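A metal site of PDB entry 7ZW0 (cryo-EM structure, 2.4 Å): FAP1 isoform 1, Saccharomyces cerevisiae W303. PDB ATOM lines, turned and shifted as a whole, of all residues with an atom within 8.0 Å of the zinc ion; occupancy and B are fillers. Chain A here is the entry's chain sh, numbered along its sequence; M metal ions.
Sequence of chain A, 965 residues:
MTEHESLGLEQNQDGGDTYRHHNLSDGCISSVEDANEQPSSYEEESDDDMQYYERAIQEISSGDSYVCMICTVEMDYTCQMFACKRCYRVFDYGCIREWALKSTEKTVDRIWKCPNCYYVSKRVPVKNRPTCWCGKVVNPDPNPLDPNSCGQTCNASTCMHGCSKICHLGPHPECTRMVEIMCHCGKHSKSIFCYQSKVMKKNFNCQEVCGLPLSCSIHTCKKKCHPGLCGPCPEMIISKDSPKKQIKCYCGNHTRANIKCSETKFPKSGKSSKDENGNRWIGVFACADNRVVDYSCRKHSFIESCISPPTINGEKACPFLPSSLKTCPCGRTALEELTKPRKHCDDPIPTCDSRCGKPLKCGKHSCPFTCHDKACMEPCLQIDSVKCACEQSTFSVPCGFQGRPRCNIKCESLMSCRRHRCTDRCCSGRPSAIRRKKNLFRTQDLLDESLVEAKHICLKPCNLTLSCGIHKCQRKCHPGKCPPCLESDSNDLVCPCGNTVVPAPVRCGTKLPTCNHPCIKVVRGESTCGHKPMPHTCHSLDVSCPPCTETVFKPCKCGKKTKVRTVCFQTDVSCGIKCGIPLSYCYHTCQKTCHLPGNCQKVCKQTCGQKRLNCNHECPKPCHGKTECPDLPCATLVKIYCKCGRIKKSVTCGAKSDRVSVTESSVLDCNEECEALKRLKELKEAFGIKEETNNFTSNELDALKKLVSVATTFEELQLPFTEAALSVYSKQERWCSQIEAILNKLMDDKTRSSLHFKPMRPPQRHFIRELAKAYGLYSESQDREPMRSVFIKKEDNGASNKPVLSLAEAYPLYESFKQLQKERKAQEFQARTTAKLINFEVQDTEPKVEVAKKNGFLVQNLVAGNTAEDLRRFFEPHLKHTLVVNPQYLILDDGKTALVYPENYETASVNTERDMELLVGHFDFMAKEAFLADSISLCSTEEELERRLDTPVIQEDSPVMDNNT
The side-chain sulfur (SG) of Cys 114 binds the zinc ion (2.0 Å). SG of Cys 87 binds the zinc ion (2.4 Å). The zinc ion is bound by the side-chain sulfur (SG) of Cys 84 (2.5 Å). The zinc ion is bound by SG of Cys 117, 2.6 Å away. The zinc ion has four donor atoms within binding distance.
N of Cys 114 is in hydrogen-bond range of O of Tyr 119 (2.7 Å). The side-chain sulfur (SG) of Cys 87 lies close to the backbone NH (N) of Arg 89, 3.4 Å away. SG of Cys 84 sits close to N of Arg 86.
Four residues have an atom within 4 Å of the zinc ion: Cys 84, Cys 87, Cys 114 and Cys 117. The nearest printed residue that does not touch the zinc ion is Phe 91 (4.5 Å).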
ATOM      1  N   MET A  69     -11.780 -27.744 -16.738  1.00  0.00           N
ATOM      2  CA  MET A  69     -11.509 -29.028 -17.386  1.00  0.00           C
ATOM      3  C   MET A  69     -11.741 -30.285 -16.560  1.00  0.00           C
ATOM      4  O   MET A  69     -12.300 -31.255 -17.067  1.00  0.00           O
ATOM      5  CB  MET A  69     -10.089 -29.033 -17.955  1.00  0.00           C
ATOM      6  CG  MET A  69      -9.876 -28.003 -19.047  1.00  0.00           C
ATOM      7  SD  MET A  69      -8.262 -28.116 -19.850  1.00  0.00           S
ATOM      8  CE  MET A  69      -8.363 -29.745 -20.582  1.00  0.00           C
ATOM      9  N   PHE A  82      -7.543 -21.348 -11.804  1.00  0.00           N
ATOM     10  CA  PHE A  82      -6.100 -21.629 -11.743  1.00  0.00           C
ATOM     11  C   PHE A  82      -5.461 -21.481 -13.126  1.00  0.00           C
ATOM     12  O   PHE A  82      -6.020 -21.968 -14.111  1.00  0.00           O
ATOM     13  CB  PHE A  82      -5.846 -23.028 -11.224  1.00  0.00           C
ATOM     14  CG  PHE A  82      -4.390 -23.407 -11.206  1.00  0.00           C
ATOM     15  CD1 PHE A  82      -3.558 -22.920 -10.218  1.00  0.00           C
ATOM     16  CD2 PHE A  82      -3.867 -24.252 -12.161  1.00  0.00           C
ATOM     17  CE1 PHE A  82      -2.213 -23.259 -10.190  1.00  0.00           C
ATOM     18  CE2 PHE A  82      -2.531 -24.590 -12.155  1.00  0.00           C
ATOM     19  CZ  PHE A  82      -1.708 -24.102 -11.163  1.00  0.00           C
ATOM     20  N   ALA A  83      -4.324 -20.812 -13.208  1.00  0.00           N
ATOM     21  CA  ALA A  83      -3.690 -20.576 -14.500  1.00  0.00           C
ATOM     22  C   ALA A  83      -2.332 -21.234 -14.609  1.00  0.00           C
ATOM     23  O   ALA A  83      -1.532 -21.185 -13.675  1.00  0.00           O
ATOM     24  CB  ALA A  83      -3.593 -19.092 -14.778  1.00  0.00           C
ATOM     25  N   CYS A  84      -2.055 -21.842 -15.751  1.00  0.00           N
ATOM     26  CA  CYS A  84      -0.748 -22.445 -15.973  1.00  0.00           C
ATOM     27  C   CYS A  84      -0.094 -21.719 -17.121  1.00  0.00           C
ATOM     28  O   CYS A  84      -0.726 -21.509 -18.146  1.00  0.00           O
ATOM     29  CB  CYS A  84      -0.866 -23.936 -16.291  1.00  0.00           C
ATOM     30  SG  CYS A  84       0.677 -24.707 -16.810  1.00  0.00           S
ATOM     31  N   LYS A  85       1.162 -21.330 -16.971  1.00  0.00           N
ATOM     32  CA  LYS A  85       1.814 -20.552 -18.010  1.00  0.00           C
ATOM     33  C   LYS A  85       1.930 -21.324 -19.308  1.00  0.00           C
ATOM     34  O   LYS A  85       1.745 -20.770 -20.381  1.00  0.00           O
ATOM     35  CB  LYS A  85       3.209 -20.093 -17.547  1.00  0.00           C
ATOM     36  CG  LYS A  85       3.208 -18.898 -16.593  1.00  0.00           C
ATOM     37  CD  LYS A  85       2.922 -19.302 -15.150  1.00  0.00           C
ATOM     38  CE  LYS A  85       1.548 -18.854 -14.707  1.00  0.00           C
ATOM     39  NZ  LYS A  85       1.136 -19.516 -13.439  1.00  0.00           N
ATOM     40  N   ARG A  86       2.225 -22.613 -19.220  1.00  0.00           N
ATOM     41  CA  ARG A  86       2.421 -23.401 -20.426  1.00  0.00           C
ATOM     42  C   ARG A  86       1.155 -23.485 -21.289  1.00  0.00           C
ATOM     43  O   ARG A  86       1.229 -23.337 -22.511  1.00  0.00           O
ATOM     44  CB  ARG A  86       2.935 -24.801 -20.069  1.00  0.00           C
ATOM     45  CG  ARG A  86       3.566 -25.540 -21.240  1.00  0.00           C
ATOM     46  CD  ARG A  86       4.794 -24.811 -21.750  1.00  0.00           C
ATOM     47  NE  ARG A  86       5.172 -25.240 -23.093  1.00  0.00           N
ATOM     48  CZ  ARG A  86       4.765 -24.648 -24.213  1.00  0.00           C
ATOM     49  NH1 ARG A  86       3.970 -23.592 -24.150  1.00  0.00           N
ATOM     50  NH2 ARG A  86       5.152 -25.111 -25.395  1.00  0.00           N
ATOM     51  N   CYS A  87       0.005 -23.699 -20.665  1.00  0.00           N
ATOM     52  CA  CYS A  87      -1.240 -23.788 -21.425  1.00  0.00           C
ATOM     53  C   CYS A  87      -2.069 -22.522 -21.428  1.00  0.00           C
ATOM     54  O   CYS A  87      -3.016 -22.421 -22.209  1.00  0.00           O
ATOM     55  CB  CYS A  87      -2.106 -24.914 -20.875  1.00  0.00           C
ATOM     56  SG  CYS A  87      -2.813 -24.555 -19.253  1.00  0.00           S
ATOM     57  N   TYR A  88      -1.715 -21.551 -20.604  1.00  0.00           N
ATOM     58  CA  TYR A  88      -2.525 -20.339 -20.467  1.00  0.00           C
ATOM     59  C   TYR A  88      -4.022 -20.622 -20.519  1.00  0.00           C
ATOM     60  O   TYR A  88      -4.770 -19.940 -21.229  1.00  0.00           O
ATOM     61  CB  TYR A  88      -2.103 -19.259 -21.465  1.00  0.00           C
ATOM     62  CG  TYR A  88      -0.902 -18.485 -20.983  1.00  0.00           C
ATOM     63  CD1 TYR A  88      -0.890 -17.935 -19.706  1.00  0.00           C
ATOM     64  CD2 TYR A  88       0.201 -18.296 -21.792  1.00  0.00           C
ATOM     65  CE1 TYR A  88       0.205 -17.226 -19.251  1.00  0.00           C
ATOM     66  CE2 TYR A  88       1.301 -17.591 -21.349  1.00  0.00           C
ATOM     67  CZ  TYR A  88       1.301 -17.063 -20.068  1.00  0.00           C
ATOM     68  OH  TYR A  88       2.392 -16.357 -19.621  1.00  0.00           O
ATOM     69  N   ARG A  89      -4.469 -21.617 -19.761  1.00  0.00           N
ATOM     70  CA  ARG A  89      -5.871 -21.973 -19.724  1.00  0.00           C
ATOM     71  C   ARG A  89      -6.308 -21.981 -18.264  1.00  0.00           C
ATOM     72  O   ARG A  89      -5.475 -22.149 -17.370  1.00  0.00           O
ATOM     73  CB  ARG A  89      -6.063 -23.344 -20.385  1.00  0.00           C
ATOM     74  CG  ARG A  89      -7.310 -24.126 -20.010  1.00  0.00           C
ATOM     75  CD  ARG A  89      -8.368 -24.067 -21.095  1.00  0.00           C
ATOM     76  NE  ARG A  89      -9.610 -24.705 -20.674  1.00  0.00           N
ATOM     77  CZ  ARG A  89     -10.678 -24.869 -21.457  1.00  0.00           C
ATOM     78  NH1 ARG A  89     -10.640 -24.452 -22.713  1.00  0.00           N
ATOM     79  NH2 ARG A  89     -11.770 -25.448 -20.979  1.00  0.00           N
ATOM     80  N   VAL A  90      -7.592 -21.798 -17.997  1.00  0.00           N
ATOM     81  CA  VAL A  90      -8.079 -21.739 -16.622  1.00  0.00           C
ATOM     82  C   VAL A  90      -9.061 -22.835 -16.226  1.00  0.00           C
ATOM     83  O   VAL A  90      -9.954 -23.195 -17.005  1.00  0.00           O
ATOM     84  CB  VAL A  90      -8.639 -20.346 -16.306  1.00  0.00           C
ATOM     85  CG1 VAL A  90      -9.720 -20.385 -15.254  1.00  0.00           C
ATOM     86  CG2 VAL A  90      -7.512 -19.429 -15.886  1.00  0.00           C
ATOM     87  N   PHE A  91      -8.876 -23.415 -15.042  1.00  0.00           N
ATOM     88  CA  PHE A  91      -9.780 -24.451 -14.556  1.00  0.00           C
ATOM     89  C   PHE A  91     -10.206 -24.007 -13.174  1.00  0.00           C
ATOM     90  O   PHE A  91      -9.635 -23.074 -12.629  1.00  0.00           O
ATOM     91  CB  PHE A  91      -9.050 -25.790 -14.456  1.00  0.00           C
ATOM     92  CG  PHE A  91      -7.753 -25.833 -15.203  1.00  0.00           C
ATOM     93  CD1 PHE A  91      -6.574 -25.410 -14.593  1.00  0.00           C
ATOM     94  CD2 PHE A  91      -7.700 -26.292 -16.508  1.00  0.00           C
ATOM     95  CE1 PHE A  91      -5.374 -25.446 -15.285  1.00  0.00           C
ATOM     96  CE2 PHE A  91      -6.509 -26.336 -17.192  1.00  0.00           C
ATOM     97  CZ  PHE A  91      -5.339 -25.902 -16.583  1.00  0.00           C
ATOM     98  N   ILE A  96      -8.783 -28.463 -10.095  1.00  0.00           N
ATOM     99  CA  ILE A  96      -7.451 -28.777 -10.575  1.00  0.00           C
ATOM    100  C   ILE A  96      -6.557 -29.289  -9.436  1.00  0.00           C
ATOM    101  O   ILE A  96      -5.655 -30.090  -9.681  1.00  0.00           O
ATOM    102  CB  ILE A  96      -6.806 -27.579 -11.312  1.00  0.00           C
ATOM    103  CG1 ILE A  96      -5.701 -28.054 -12.260  1.00  0.00           C
ATOM    104  CG2 ILE A  96      -6.232 -26.554 -10.340  1.00  0.00           C
ATOM    105  CD1 ILE A  96      -6.192 -28.982 -13.346  1.00  0.00           C
ATOM    106  N   TRP A 112       2.572 -33.150 -10.142  1.00  0.00           N
ATOM    107  CA  TRP A 112       1.246 -32.835 -10.667  1.00  0.00           C
ATOM    108  C   TRP A 112       1.279 -32.511 -12.167  1.00  0.00           C
ATOM    109  O   TRP A 112       2.263 -31.979 -12.655  1.00  0.00           O
ATOM    110  CB  TRP A 112       0.628 -31.684  -9.870  1.00  0.00           C
ATOM    111  CG  TRP A 112       0.684 -30.355 -10.539  1.00  0.00           C
ATOM    112  CD1 TRP A 112       1.726 -29.480 -10.545  1.00  0.00           C
ATOM    113  CD2 TRP A 112      -0.367 -29.733 -11.304  1.00  0.00           C
ATOM    114  NE1 TRP A 112       1.388 -28.358 -11.261  1.00  0.00           N
ATOM    115  CE2 TRP A 112       0.114 -28.494 -11.739  1.00  0.00           C
ATOM    116  CE3 TRP A 112      -1.663 -30.120 -11.656  1.00  0.00           C
ATOM    117  CZ2 TRP A 112      -0.649 -27.630 -12.509  1.00  0.00           C
ATOM    118  CZ3 TRP A 112      -2.412 -29.263 -12.417  1.00  0.00           C
ATOM    119  CH2 TRP A 112      -1.917 -28.030 -12.844  1.00  0.00           C
ATOM    120  N   LYS A 113       0.205 -32.817 -12.899  1.00  0.00           N
ATOM    121  CA  LYS A 113       0.220 -32.598 -14.361  1.00  0.00           C
ATOM    122  C   LYS A 113      -0.876 -31.651 -14.830  1.00  0.00           C
ATOM    123  O   LYS A 113      -2.002 -31.740 -14.367  1.00  0.00           O
ATOM    124  CB  LYS A 113       0.090 -33.941 -15.091  1.00  0.00           C
ATOM    125  CG  LYS A 113       0.346 -33.854 -16.589  1.00  0.00           C
ATOM    126  CD  LYS A 113       0.672 -35.220 -17.160  1.00  0.00           C
ATOM    127  CE  LYS A 113       1.289 -35.082 -18.540  1.00  0.00           C
ATOM    128  NZ  LYS A 113       1.776 -36.398 -19.056  1.00  0.00           N
ATOM    129  N   CYS A 114      -0.551 -30.762 -15.745  1.00  0.00           N
ATOM    130  CA  CYS A 114      -1.551 -29.863 -16.285  1.00  0.00           C
ATOM    131  C   CYS A 114      -2.104 -30.436 -17.571  1.00  0.00           C
ATOM    132  O   CYS A 114      -1.360 -30.631 -18.525  1.00  0.00           O
ATOM    133  CB  CYS A 114      -0.956 -28.486 -16.541  1.00  0.00           C
ATOM    134  SG  CYS A 114      -2.160 -27.294 -17.156  1.00  0.00           S
ATOM    135  N   PRO A 115      -3.413 -30.696 -17.627  1.00  0.00           N
ATOM    136  CA  PRO A 115      -4.016 -31.352 -18.798  1.00  0.00           C
ATOM    137  C   PRO A 115      -3.992 -30.606 -20.131  1.00  0.00           C
ATOM    138  O   PRO A 115      -3.732 -31.245 -21.150  1.00  0.00           O
ATOM    139  CB  PRO A 115      -5.481 -31.546 -18.386  1.00  0.00           C
ATOM    140  CG  PRO A 115      -5.503 -31.386 -16.895  1.00  0.00           C
ATOM    141  CD  PRO A 115      -4.415 -30.412 -16.583  1.00  0.00           C
ATOM    142  N   ASN A 116      -4.253 -29.311 -20.141  1.00  0.00           N
ATOM    143  CA  ASN A 116      -4.343 -28.604 -21.422  1.00  0.00           C
ATOM    144  C   ASN A 116      -3.040 -28.613 -22.190  1.00  0.00           C
ATOM    145  O   ASN A 116      -3.030 -28.822 -23.407  1.00  0.00           O
ATOM    146  CB  ASN A 116      -4.837 -27.171 -21.220  1.00  0.00           C
ATOM    147  CG  ASN A 116      -5.399 -26.568 -22.503  1.00  0.00           C
ATOM    148  OD1 ASN A 116      -6.280 -27.157 -23.135  1.00  0.00           O
ATOM    149  ND2 ASN A 116      -4.909 -25.397 -22.872  1.00  0.00           N
ATOM    150  N   CYS A 117      -1.930 -28.401 -21.500  1.00  0.00           N
ATOM    151  CA  CYS A 117      -0.629 -28.466 -22.153  1.00  0.00           C
ATOM    152  C   CYS A 117      -0.049 -29.850 -22.007  1.00  0.00           C
ATOM    153  O   CYS A 117       1.062 -30.102 -22.485  1.00  0.00           O
ATOM    154  CB  CYS A 117       0.322 -27.436 -21.560  1.00  0.00           C
ATOM    155  SG  CYS A 117       0.254 -27.347 -19.766  1.00  0.00           S
ATOM    156  N   TYR A 118      -0.772 -30.742 -21.339  1.00  0.00           N
ATOM    157  CA  TYR A 118      -0.274 -32.092 -21.085  1.00  0.00           C
ATOM    158  C   TYR A 118       1.134 -31.953 -20.550  1.00  0.00           C
ATOM    159  O   TYR A 118       2.045 -32.654 -20.984  1.00  0.00           O
ATOM    160  CB  TYR A 118      -0.313 -32.945 -22.365  1.00  0.00           C
ATOM    161  CG  TYR A 118      -0.364 -34.425 -22.110  1.00  0.00           C
ATOM    162  CD1 TYR A 118      -1.409 -34.996 -21.391  1.00  0.00           C
ATOM    163  CD2 TYR A 118       0.628 -35.267 -22.597  1.00  0.00           C
ATOM    164  CE1 TYR A 118      -1.453 -36.352 -21.155  1.00  0.00           C
ATOM    165  CE2 TYR A 118       0.589 -36.628 -22.373  1.00  0.00           C
ATOM    166  CZ  TYR A 118      -0.463 -37.167 -21.654  1.00  0.00           C
ATOM    167  OH  TYR A 118      -0.511 -38.526 -21.426  1.00  0.00           O
ATOM    168  N   TYR A 119       1.324 -31.037 -19.606  1.00  0.00           N
ATOM    169  CA  TYR A 119       2.663 -30.778 -19.088  1.00  0.00           C
ATOM    170  C   TYR A 119       2.723 -30.992 -17.604  1.00  0.00           C
ATOM    171  O   TYR A 119       1.913 -30.446 -16.858  1.00  0.00           O
ATOM    172  CB  TYR A 119       3.101 -29.363 -19.495  1.00  0.00           C
ATOM    173  CG  TYR A 119       3.797 -28.521 -18.439  1.00  0.00           C
ATOM    174  CD1 TYR A 119       3.077 -27.705 -17.582  1.00  0.00           C
ATOM    175  CD2 TYR A 119       5.181 -28.503 -18.344  1.00  0.00           C
ATOM    176  CE1 TYR A 119       3.701 -26.929 -16.629  1.00  0.00           C
ATOM    177  CE2 TYR A 119       5.814 -27.729 -17.395  1.00  0.00           C
ATOM    178  CZ  TYR A 119       5.075 -26.951 -16.545  1.00  0.00           C
ATOM    179  OH  TYR A 119       5.699 -26.175 -15.592  1.00  0.00           O
ATOM    180  N   VAL A 120       3.661 -31.817 -17.157  1.00  0.00           N
ATOM    181  CA  VAL A 120       3.818 -32.038 -15.727  1.00  0.00           C
ATOM    182  C   VAL A 120       4.555 -30.888 -15.081  1.00  0.00           C
ATOM    183  O   VAL A 120       5.457 -30.313 -15.673  1.00  0.00           O
ATOM    184  CB  VAL A 120       4.590 -33.338 -15.459  1.00  0.00           C
ATOM    185  CG1 VAL A 120       3.746 -34.291 -14.618  1.00  0.00           C
ATOM    186  CG2 VAL A 120       4.978 -33.993 -16.765  1.00  0.00           C
ATOM    187  N   SER A 121       4.192 -30.558 -13.854  1.00  0.00           N
ATOM    188  CA  SER A 121       4.891 -29.510 -13.113  1.00  0.00           C
ATOM    189  C   SER A 121       5.209 -30.070 -11.746  1.00  0.00           C
ATOM    190  O   SER A 121       4.654 -31.108 -11.365  1.00  0.00           O
ATOM    191  CB  SER A 121       4.072 -28.222 -13.046  1.00  0.00           C
ATOM    192  OG  SER A 121       4.801 -27.179 -12.414  1.00  0.00           O
HETATM  193 ZN    ZN M   1      -1.127 -25.839 -18.162  1.00  0.00          ZN
